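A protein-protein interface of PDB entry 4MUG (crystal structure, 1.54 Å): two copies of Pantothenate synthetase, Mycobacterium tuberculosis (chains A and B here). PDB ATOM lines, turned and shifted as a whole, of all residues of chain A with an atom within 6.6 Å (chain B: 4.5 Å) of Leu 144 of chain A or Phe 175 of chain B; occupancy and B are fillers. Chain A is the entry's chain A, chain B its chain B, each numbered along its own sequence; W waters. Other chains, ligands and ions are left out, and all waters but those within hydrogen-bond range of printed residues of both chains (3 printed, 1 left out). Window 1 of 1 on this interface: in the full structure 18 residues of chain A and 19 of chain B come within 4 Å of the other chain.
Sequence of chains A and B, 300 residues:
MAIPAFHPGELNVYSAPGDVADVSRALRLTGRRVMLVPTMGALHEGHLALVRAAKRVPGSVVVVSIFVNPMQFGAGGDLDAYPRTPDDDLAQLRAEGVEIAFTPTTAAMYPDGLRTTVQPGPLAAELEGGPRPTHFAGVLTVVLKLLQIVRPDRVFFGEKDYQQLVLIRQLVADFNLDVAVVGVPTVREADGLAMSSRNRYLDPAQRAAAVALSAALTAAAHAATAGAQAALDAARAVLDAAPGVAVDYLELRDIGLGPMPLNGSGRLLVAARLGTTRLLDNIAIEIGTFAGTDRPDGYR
OG1 of Thr 116 of chain A is in hydrogen-bond range of OD2 of Asp 174 of chain B. The side-chain amino group (NZ) of Lys 145 of chain A is in hydrogen-bond range of the backbone carbonyl oxygen (O) of Asp 174 of chain B (2.9 Å). NZ of Lys 145 of chain A sits at hydrogen-bond distance from OD1 of Asn 176 of chain B (2.8 Å).
Of chain B, only Phe 175 comes within 4 Å of Leu 144 of chain A. Of the printed residues of chain A, Phe 175 of chain B touches Thr 116 (3.5 Å), Thr 117 (3.6 Å), Val 118 (3.9 Å), Leu 144 (3.6 Å) and Gln 148 (3.2 Å). Of the printed residues of chain B, Thr 116 of chain A touches Val 118, Leu 171, Asp 174 and Phe 175. Of the printed residues of chain B, Phe 175 of chain A touches Val 118 and Leu 144. Of the printed residues of chain A, Asp 174 of chain B touches Thr 116 (2.7 Å) and Lys 145 (2.9 Å). Printed residues of chain A within 4 Å of Val 118 of chain B: Thr 116 (3.4 Å), Thr 117 (3.7 Å) and Phe 175 (3.9 Å). Leu 177 of chain A touches none of the printed residues of chain B. The nearest printed residue of chain A that does not touch Phe 175 of chain B is Lys 145 of chain A (4.02 Å). The nearest printed residue of chain A that does not touch Val 118 of chain B is Gln 119 of chain A (4.7 Å).
Thr 116 of chain A touches Val 118 of chain B. Leu 171 of chain B touches Thr 116 of chain A (N to OG1, 3.8 Å). Thr 117 of chain A touches Val 118 of chain B (O to C, 3.7 Å). O of Thr 117 of chain A touches CZ of Phe 175 of chain B, 3.6 Å away. Val 118 of chain A touches Phe 175 of chain B (CG2 to CZ, 3.9 Å). Phe 175 of chain B touches Leu 144 of chain A. Gln 148 of chain A touches Phe 175 of chain B. Gln 148 of chain A touches Asn 176 of chain B. Ile 149 of chain A touches Asn 176 of chain B (CG1 to CG, 3.7 Å). Val 118 of chain B touches Phe 175 of chain A (CG2 to CZ, 3.9 Å).
Water W2 lies within hydrogen-bond range of O of Asn 176 of chain B and O of Gln 148 of chain A. Water W1 lies within hydrogen-bond range of O of Ala 173 of chain B (2.8 Å) and NZ of Lys 145 of chain A (3.5 Å). Water W3 bridges ND2 of Asn 176 of chain B (2.9 Å) and NZ of Lys 145 of chain A (3.2 Å).
O of Val 172 of chain B lies within hydrogen-bond range of N of Leu 177 of chain B. N of Val 118 of chain A sits at hydrogen-bond distance from OG1 of Thr 141 of chain A, 3.0 Å away.
Val 118 of chain A touches Phe 175 of chain B, and with the chains exchanged Phe 175 of chain A touches Val 118 of chain B. Leu 144 of chain A touches Phe 175 of chain B, and with the chains exchanged Phe 175 of chain A touches Leu 144 of chain B. Positions printed for both chains: 118, 144, 171, 175 and 177. Of the 16 pairs that touch across the chains among the printed residues, 4 have their exchanged pair printed and touching as well.
Hydrophobic or aromatic side chains of chain B within 4 Å of the printed part of chain A: Val 118, Leu 144, Phe 175 and Leu 177. Hydrophobic or aromatic side chains of chain A within 4 Å of the printed part of chain B: Val 118, Leu 144, Ile 149 and Phe 175. Among the printed residues, 16 pairs touch across the chains. Among the printed residues, no Asp or Glu carboxylate lies within 4 Å of a Lys or Arg side-chain nitrogen of the other chain.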
ATOM      1  N   THR A 116      35.507   9.933  27.170  1.00  0.00           N
ATOM      2  CA  THR A 116      34.219   9.424  27.725  1.00  0.00           C
ATOM      3  C   THR A 116      33.114   9.803  26.757  1.00  0.00           C
ATOM      4  O   THR A 116      33.052  10.973  26.246  1.00  0.00           O
ATOM      5  CB  THR A 116      33.960  10.121  29.078  1.00  0.00           C
ATOM      6  OG1 THR A 116      35.151  10.190  29.886  1.00  0.00           O
ATOM      7  CG2 THR A 116      32.823   9.417  29.930  1.00  0.00           C
ATOM      8  N   THR A 117      32.188   8.876  26.539  1.00  0.00           N
ATOM      9  CA  THR A 117      31.060   9.161  25.642  1.00  0.00           C
ATOM     10  C   THR A 117      29.797   8.532  26.209  1.00  0.00           C
ATOM     11  O   THR A 117      29.831   7.791  27.269  1.00  0.00           O
ATOM     12  CB  THR A 117      31.236   8.627  24.221  1.00  0.00           C
ATOM     13  OG1 THR A 117      31.438   7.207  24.334  1.00  0.00           O
ATOM     14  CG2 THR A 117      32.493   9.085  23.591  1.00  0.00           C
ATOM     15  N   VAL A 118      28.694   8.978  25.680  1.00  0.00           N
ATOM     16  CA  VAL A 118      27.358   8.397  25.998  1.00  0.00           C
ATOM     17  C   VAL A 118      27.141   7.177  25.113  1.00  0.00           C
ATOM     18  O   VAL A 118      27.198   7.221  23.895  1.00  0.00           O
ATOM     19  CB  VAL A 118      26.213   9.385  25.852  1.00  0.00           C
ATOM     20  CG1 VAL A 118      24.875   8.693  26.148  1.00  0.00           C
ATOM     21  CG2 VAL A 118      26.476  10.621  26.762  1.00  0.00           C
ATOM     22  N   GLN A 119      26.764   6.087  25.804  1.00  0.00           N
ATOM     23  CA  GLN A 119      26.373   4.918  25.040  1.00  0.00           C
ATOM     24  C   GLN A 119      24.802   4.819  25.127  1.00  0.00           C
ATOM     25  O   GLN A 119      24.209   4.595  26.221  1.00  0.00           O
ATOM     26  CB  GLN A 119      26.973   3.691  25.709  1.00  0.00           C
ATOM     27  CG  GLN A 119      26.417   2.420  25.093  1.00  0.00           C
ATOM     28  CD  GLN A 119      27.381   1.933  24.084  1.00  0.00           C
ATOM     29  OE1 GLN A 119      28.120   0.992  24.346  1.00  0.00           O
ATOM     30  NE2 GLN A 119      27.475   2.639  22.962  1.00  0.00           N
ATOM     31  N   VAL A 139      25.379  12.103  18.921  1.00  0.00           N
ATOM     32  CA  VAL A 139      24.345  13.124  19.216  1.00  0.00           C
ATOM     33  C   VAL A 139      24.174  13.260  20.732  1.00  0.00           C
ATOM     34  O   VAL A 139      24.149  14.382  21.304  1.00  0.00           O
ATOM     35  CB  VAL A 139      22.912  12.728  18.681  1.00  0.00           C
ATOM     36  CG1 VAL A 139      21.905  13.785  19.150  1.00  0.00           C
ATOM     37  CG2 VAL A 139      22.970  12.695  17.122  1.00  0.00           C
ATOM     38  N   LEU A 140      24.012  12.139  21.414  1.00  0.00           N
ATOM     39  CA  LEU A 140      23.710  12.266  22.818  1.00  0.00           C
ATOM     40  C   LEU A 140      24.915  12.791  23.661  1.00  0.00           C
ATOM     41  O   LEU A 140      24.732  13.419  24.686  1.00  0.00           O
ATOM     42  CB  LEU A 140      23.256  10.884  23.376  1.00  0.00           C
ATOM     43  CG  LEU A 140      21.870  10.288  23.062  1.00  0.00           C
ATOM     44  CD1 LEU A 140      21.458   9.121  23.999  1.00  0.00           C
ATOM     45  CD2 LEU A 140      20.828  11.348  22.894  1.00  0.00           C
ATOM     46  N   THR A 141      26.137  12.496  23.208  1.00  0.00           N
ATOM     47  CA  THR A 141      27.328  13.066  23.861  1.00  0.00           C
ATOM     48  C   THR A 141      27.354  14.581  23.738  1.00  0.00           C
ATOM     49  O   THR A 141      27.561  15.264  24.721  1.00  0.00           O
ATOM     50  CB  THR A 141      28.600  12.430  23.262  1.00  0.00           C
ATOM     51  OG1 THR A 141      28.622  10.984  23.456  1.00  0.00           O
ATOM     52  CG2 THR A 141      29.769  12.970  23.910  1.00  0.00           C
ATOM     53  N   VAL A 142      27.162  15.049  22.486  1.00  0.00           N
ATOM     54  CA  VAL A 142      27.120  16.504  22.393  1.00  0.00           C
ATOM     55  C   VAL A 142      25.963  17.153  23.134  1.00  0.00           C
ATOM     56  O   VAL A 142      26.171  18.225  23.754  1.00  0.00           O
ATOM     57  CB  VAL A 142      27.267  16.996  20.918  1.00  0.00           C
ATOM     58  CG1 VAL A 142      25.929  17.024  20.176  1.00  0.00           C
ATOM     59  CG2 VAL A 142      27.964  18.409  20.900  1.00  0.00           C
ATOM     60  N   VAL A 143      24.758  16.534  23.101  1.00  0.00           N
ATOM     61  CA  VAL A 143      23.666  17.200  23.744  1.00  0.00           C
ATOM     62  C   VAL A 143      23.886  17.162  25.292  1.00  0.00           C
ATOM     63  O   VAL A 143      23.634  18.167  25.966  1.00  0.00           O
ATOM     64  CB  VAL A 143      22.374  16.475  23.374  1.00  0.00           C
ATOM     65  CG1 VAL A 143      21.240  16.852  24.343  1.00  0.00           C
ATOM     66  CG2 VAL A 143      21.986  16.811  21.935  1.00  0.00           C
ATOM     67  N   LEU A 144      24.479  16.115  25.814  1.00  0.00           N
ATOM     68  CA  LEU A 144      24.830  16.175  27.201  1.00  0.00           C
ATOM     69  C   LEU A 144      25.805  17.275  27.584  1.00  0.00           C
ATOM     70  O   LEU A 144      25.553  17.991  28.502  1.00  0.00           O
ATOM     71  CB  LEU A 144      25.363  14.756  27.617  1.00  0.00           C
ATOM     72  CG  LEU A 144      25.788  14.595  29.102  1.00  0.00           C
ATOM     73  CD1 LEU A 144      24.553  14.807  30.052  1.00  0.00           C
ATOM     74  CD2 LEU A 144      26.404  13.190  29.324  1.00  0.00           C
ATOM     75  N   LYS A 145      26.813  17.412  26.724  1.00  0.00           N
ATOM     76  CA  LYS A 145      27.764  18.486  27.068  1.00  0.00           C
ATOM     77  C   LYS A 145      27.059  19.782  26.991  1.00  0.00           C
ATOM     78  O   LYS A 145      27.340  20.615  27.869  1.00  0.00           O
ATOM     79  CB  LYS A 145      28.898  18.376  26.017  1.00  0.00           C
ATOM     80  CG  LYS A 145      29.818  17.172  26.295  1.00  0.00           C
ATOM     81  CD  LYS A 145      30.749  16.753  25.132  1.00  0.00           C
ATOM     82  CE  LYS A 145      31.787  17.877  24.858  1.00  0.00           C
ATOM     83  NZ  LYS A 145      32.756  18.109  25.944  1.00  0.00           N
ATOM     84  N   LEU A 146      26.288  20.052  25.946  1.00  0.00           N
ATOM     85  CA  LEU A 146      25.595  21.341  25.878  1.00  0.00           C
ATOM     86  C   LEU A 146      24.661  21.615  27.089  1.00  0.00           C
ATOM     87  O   LEU A 146      24.654  22.749  27.620  1.00  0.00           O
ATOM     88  CB  LEU A 146      24.802  21.384  24.608  1.00  0.00           C
ATOM     89  CG  LEU A 146      25.641  21.413  23.285  1.00  0.00           C
ATOM     90  CD1 LEU A 146      24.753  21.257  22.074  1.00  0.00           C
ATOM     91  CD2 LEU A 146      26.419  22.756  23.179  1.00  0.00           C
ATOM     92  N   LEU A 147      23.996  20.558  27.580  1.00  0.00           N
ATOM     93  CA  LEU A 147      23.092  20.631  28.716  1.00  0.00           C
ATOM     94  C   LEU A 147      23.933  21.006  29.937  1.00  0.00           C
ATOM     95  O   LEU A 147      23.522  21.855  30.750  1.00  0.00           O
ATOM     96  CB  LEU A 147      22.349  19.314  28.905  1.00  0.00           C
ATOM     97  CG  LEU A 147      21.256  19.164  27.886  1.00  0.00           C
ATOM     98  CD1 LEU A 147      20.599  17.797  28.017  1.00  0.00           C
ATOM     99  CD2 LEU A 147      20.207  20.277  28.032  1.00  0.00           C
ATOM    100  N   GLN A 148      25.123  20.411  30.085  1.00  0.00           N
ATOM    101  CA  GLN A 148      26.029  20.779  31.200  1.00  0.00           C
ATOM    102  C   GLN A 148      26.636  22.122  31.173  1.00  0.00           C
ATOM    103  O   GLN A 148      26.787  22.741  32.208  1.00  0.00           O
ATOM    104  CB  GLN A 148      27.110  19.670  31.375  1.00  0.00           C
ATOM    105  CG  GLN A 148      26.413  18.297  31.557  1.00  0.00           C
ATOM    106  CD  GLN A 148      25.708  18.098  32.937  1.00  0.00           C
ATOM    107  OE1 GLN A 148      26.082  18.665  33.900  1.00  0.00           O
ATOM    108  NE2 GLN A 148      24.697  17.261  32.957  1.00  0.00           N
ATOM    109  N   ILE A 149      26.980  22.553  29.943  1.00  0.00           N
ATOM    110  CA  ILE A 149      27.634  23.817  29.881  1.00  0.00           C
ATOM    111  C   ILE A 149      26.580  24.871  30.133  1.00  0.00           C
ATOM    112  O   ILE A 149      26.887  25.895  30.860  1.00  0.00           O
ATOM    113  CB  ILE A 149      28.184  24.023  28.448  1.00  0.00           C
ATOM    114  CG1 ILE A 149      29.401  23.108  28.246  1.00  0.00           C
ATOM    115  CG2 ILE A 149      28.635  25.523  28.102  1.00  0.00           C
ATOM    116  CD1 ILE A 149      29.757  22.918  26.756  1.00  0.00           C
ATOM    117  N   LEU A 171      18.094   9.913  27.447  1.00  0.00           N
ATOM    118  CA  LEU A 171      19.273  10.481  28.108  1.00  0.00           C
ATOM    119  C   LEU A 171      18.875  11.259  29.375  1.00  0.00           C
ATOM    120  O   LEU A 171      19.497  11.055  30.447  1.00  0.00           O
ATOM    121  CB  LEU A 171      19.951  11.428  27.069  1.00  0.00           C
ATOM    122  CG  LEU A 171      21.083  12.361  27.609  1.00  0.00           C
ATOM    123  CD1 LEU A 171      22.384  11.627  27.746  1.00  0.00           C
ATOM    124  CD2 LEU A 171      21.359  13.562  26.679  1.00  0.00           C
ATOM    125  N   PHE A 175      20.027   9.613  32.965  1.00  0.00           N
ATOM    126  CA  PHE A 175      21.056  10.232  33.754  1.00  0.00           C
ATOM    127  C   PHE A 175      20.520  11.309  34.717  1.00  0.00           C
ATOM    128  O   PHE A 175      21.299  12.088  35.326  1.00  0.00           O
ATOM    129  CB  PHE A 175      22.020  10.947  32.792  1.00  0.00           C
ATOM    130  CG  PHE A 175      22.851  10.014  31.975  1.00  0.00           C
ATOM    131  CD1 PHE A 175      22.973   8.652  32.255  1.00  0.00           C
ATOM    132  CD2 PHE A 175      23.636  10.490  30.941  1.00  0.00           C
ATOM    133  CE1 PHE A 175      23.784   7.849  31.521  1.00  0.00           C
ATOM    134  CE2 PHE A 175      24.467   9.679  30.220  1.00  0.00           C
ATOM    135  CZ  PHE A 175      24.531   8.286  30.461  1.00  0.00           C
ATOM    136  N   LEU A 177      18.904  14.018  34.471  1.00  0.00           N
ATOM    137  CA  LEU A 177      19.159  15.434  34.221  1.00  0.00           C
ATOM    138  C   LEU A 177      18.015  16.309  34.615  1.00  0.00           C
ATOM    139  O   LEU A 177      16.819  15.938  34.462  1.00  0.00           O
ATOM    140  CB  LEU A 177      19.581  15.681  32.739  1.00  0.00           C
ATOM    141  CG  LEU A 177      20.634  14.714  32.165  1.00  0.00           C
ATOM    142  CD1 LEU A 177      20.973  15.048  30.646  1.00  0.00           C
ATOM    143  CD2 LEU A 177      21.935  14.689  32.938  1.00  0.00           C
ATOM    144  N   VAL B 118      27.168   5.268  30.492  1.00  0.00           N
ATOM    145  CA  VAL B 118      28.424   5.949  30.219  1.00  0.00           C
ATOM    146  C   VAL B 118      29.421   4.974  29.665  1.00  0.00           C
ATOM    147  O   VAL B 118      29.671   3.918  30.275  1.00  0.00           O
ATOM    148  CB  VAL B 118      29.017   6.652  31.425  1.00  0.00           C
ATOM    149  CG1 VAL B 118      30.393   7.368  31.032  1.00  0.00           C
ATOM    150  CG2 VAL B 118      28.056   7.674  32.034  1.00  0.00           C
ATOM    151  N   LEU B 144      27.773   9.375  37.625  1.00  0.00           N
ATOM    152  CA  LEU B 144      27.061  10.444  36.879  1.00  0.00           C
ATOM    153  C   LEU B 144      25.658  10.767  37.380  1.00  0.00           C
ATOM    154  O   LEU B 144      25.313  11.953  37.601  1.00  0.00           O
ATOM    155  CB  LEU B 144      27.100  10.260  35.336  1.00  0.00           C
ATOM    156  CG  LEU B 144      26.360  11.266  34.451  1.00  0.00           C
ATOM    157  CD1 LEU B 144      27.115  12.660  34.621  1.00  0.00           C
ATOM    158  CD2 LEU B 144      26.387  10.752  32.997  1.00  0.00           C
ATOM    159  N   LEU B 171      35.497  11.807  33.252  1.00  0.00           N
ATOM    160  CA  LEU B 171      34.047  11.989  33.123  1.00  0.00           C
ATOM    161  C   LEU B 171      33.669  13.430  33.365  1.00  0.00           C
ATOM    162  O   LEU B 171      32.905  13.996  32.552  1.00  0.00           O
ATOM    163  CB  LEU B 171      33.307  11.138  34.201  1.00  0.00           C
ATOM    164  CG  LEU B 171      31.804  11.350  34.428  1.00  0.00           C
ATOM    165  CD1 LEU B 171      31.050  10.602  33.358  1.00  0.00           C
ATOM    166  CD2 LEU B 171      31.345  10.843  35.870  1.00  0.00           C
ATOM    167  N   VAL B 172      34.210  14.050  34.415  1.00  0.00           N
ATOM    168  CA  VAL B 172      33.852  15.435  34.793  1.00  0.00           C
ATOM    169  C   VAL B 172      34.359  16.345  33.668  1.00  0.00           C
ATOM    170  O   VAL B 172      33.636  17.324  33.278  1.00  0.00           O
ATOM    171  CB  VAL B 172      34.407  15.833  36.154  1.00  0.00           C
ATOM    172  CG1 VAL B 172      34.411  17.334  36.440  1.00  0.00           C
ATOM    173  CG2 VAL B 172      33.570  15.080  37.212  1.00  0.00           C
ATOM    174  N   ALA B 173      35.585  16.155  33.218  1.00  0.00           N
ATOM    175  CA  ALA B 173      36.120  17.017  32.098  1.00  0.00           C
ATOM    176  C   ALA B 173      35.357  16.830  30.834  1.00  0.00           C
ATOM    177  O   ALA B 173      34.938  17.822  30.147  1.00  0.00           O
ATOM    178  CB  ALA B 173      37.593  16.808  31.841  1.00  0.00           C
ATOM    179  N   ASP B 174      35.142  15.575  30.448  1.00  0.00           N
ATOM    180  CA  ASP B 174      34.580  15.274  29.182  1.00  0.00           C
ATOM    181  C   ASP B 174      33.124  15.627  28.943  1.00  0.00           C
ATOM    182  O   ASP B 174      32.662  15.908  27.813  1.00  0.00           O
ATOM    183  CB  ASP B 174      34.795  13.823  28.792  1.00  0.00           C
ATOM    184  CG  ASP B 174      36.253  13.428  28.734  1.00  0.00           C
ATOM    185  OD1 ASP B 174      37.163  14.329  28.590  1.00  0.00           O
ATOM    186  OD2 ASP B 174      36.585  12.177  28.726  1.00  0.00           O
ATOM    187  N   PHE B 175      32.347  15.546  30.053  1.00  0.00           N
ATOM    188  CA  PHE B 175      30.986  15.947  29.940  1.00  0.00           C
ATOM    189  C   PHE B 175      30.703  17.319  30.552  1.00  0.00           C
ATOM    190  O   PHE B 175      29.543  17.725  30.740  1.00  0.00           O
ATOM    191  CB  PHE B 175      30.103  14.918  30.718  1.00  0.00           C
ATOM    192  CG  PHE B 175      30.029  13.577  30.059  1.00  0.00           C
ATOM    193  CD1 PHE B 175      30.374  13.335  28.733  1.00  0.00           C
ATOM    194  CD2 PHE B 175      29.550  12.533  30.838  1.00  0.00           C
ATOM    195  CE1 PHE B 175      30.287  12.064  28.134  1.00  0.00           C
ATOM    196  CE2 PHE B 175      29.435  11.258  30.251  1.00  0.00           C
ATOM    197  CZ  PHE B 175      29.752  11.029  28.915  1.00  0.00           C
ATOM    198  N   ASN B 176      31.810  18.078  30.851  1.00  0.00           N
ATOM    199  CA  ASN B 176      31.647  19.467  31.306  1.00  0.00           C
ATOM    200  C   ASN B 176      30.805  19.647  32.567  1.00  0.00           C
ATOM    201  O   ASN B 176      30.039  20.576  32.741  1.00  0.00           O
ATOM    202  CB  ASN B 176      30.968  20.316  30.181  1.00  0.00           C
ATOM    203  CG  ASN B 176      31.733  20.301  28.845  1.00  0.00           C
ATOM    204  OD1 ASN B 176      31.408  19.452  27.981  1.00  0.00           O
ATOM    205  ND2 ASN B 176      32.815  21.119  28.725  1.00  0.00           N
ATOM    206  N   LEU B 177      31.009  18.651  33.466  1.00  0.00           N
ATOM    207  CA  LEU B 177      30.267  18.730  34.725  1.00  0.00           C
ATOM    208  C   LEU B 177      30.801  19.840  35.653  1.00  0.00           C
ATOM    209  O   LEU B 177      31.992  20.117  35.687  1.00  0.00           O
ATOM    210  CB  LEU B 177      30.362  17.420  35.443  1.00  0.00           C
ATOM    211  CG  LEU B 177      29.881  16.188  34.628  1.00  0.00           C
ATOM    212  CD1 LEU B 177      29.932  14.928  35.568  1.00  0.00           C
ATOM    213  CD2 LEU B 177      28.530  16.174  33.962  1.00  0.00           C
HETATM  214  O   HOH W   1      35.792  18.390  27.573  1.00  0.00           O
HETATM  215  O   HOH W   2      29.930  23.186  33.115  1.00  0.00           O
HETATM  216  O   HOH W   3      34.711  20.524  26.564  1.00  0.00           O
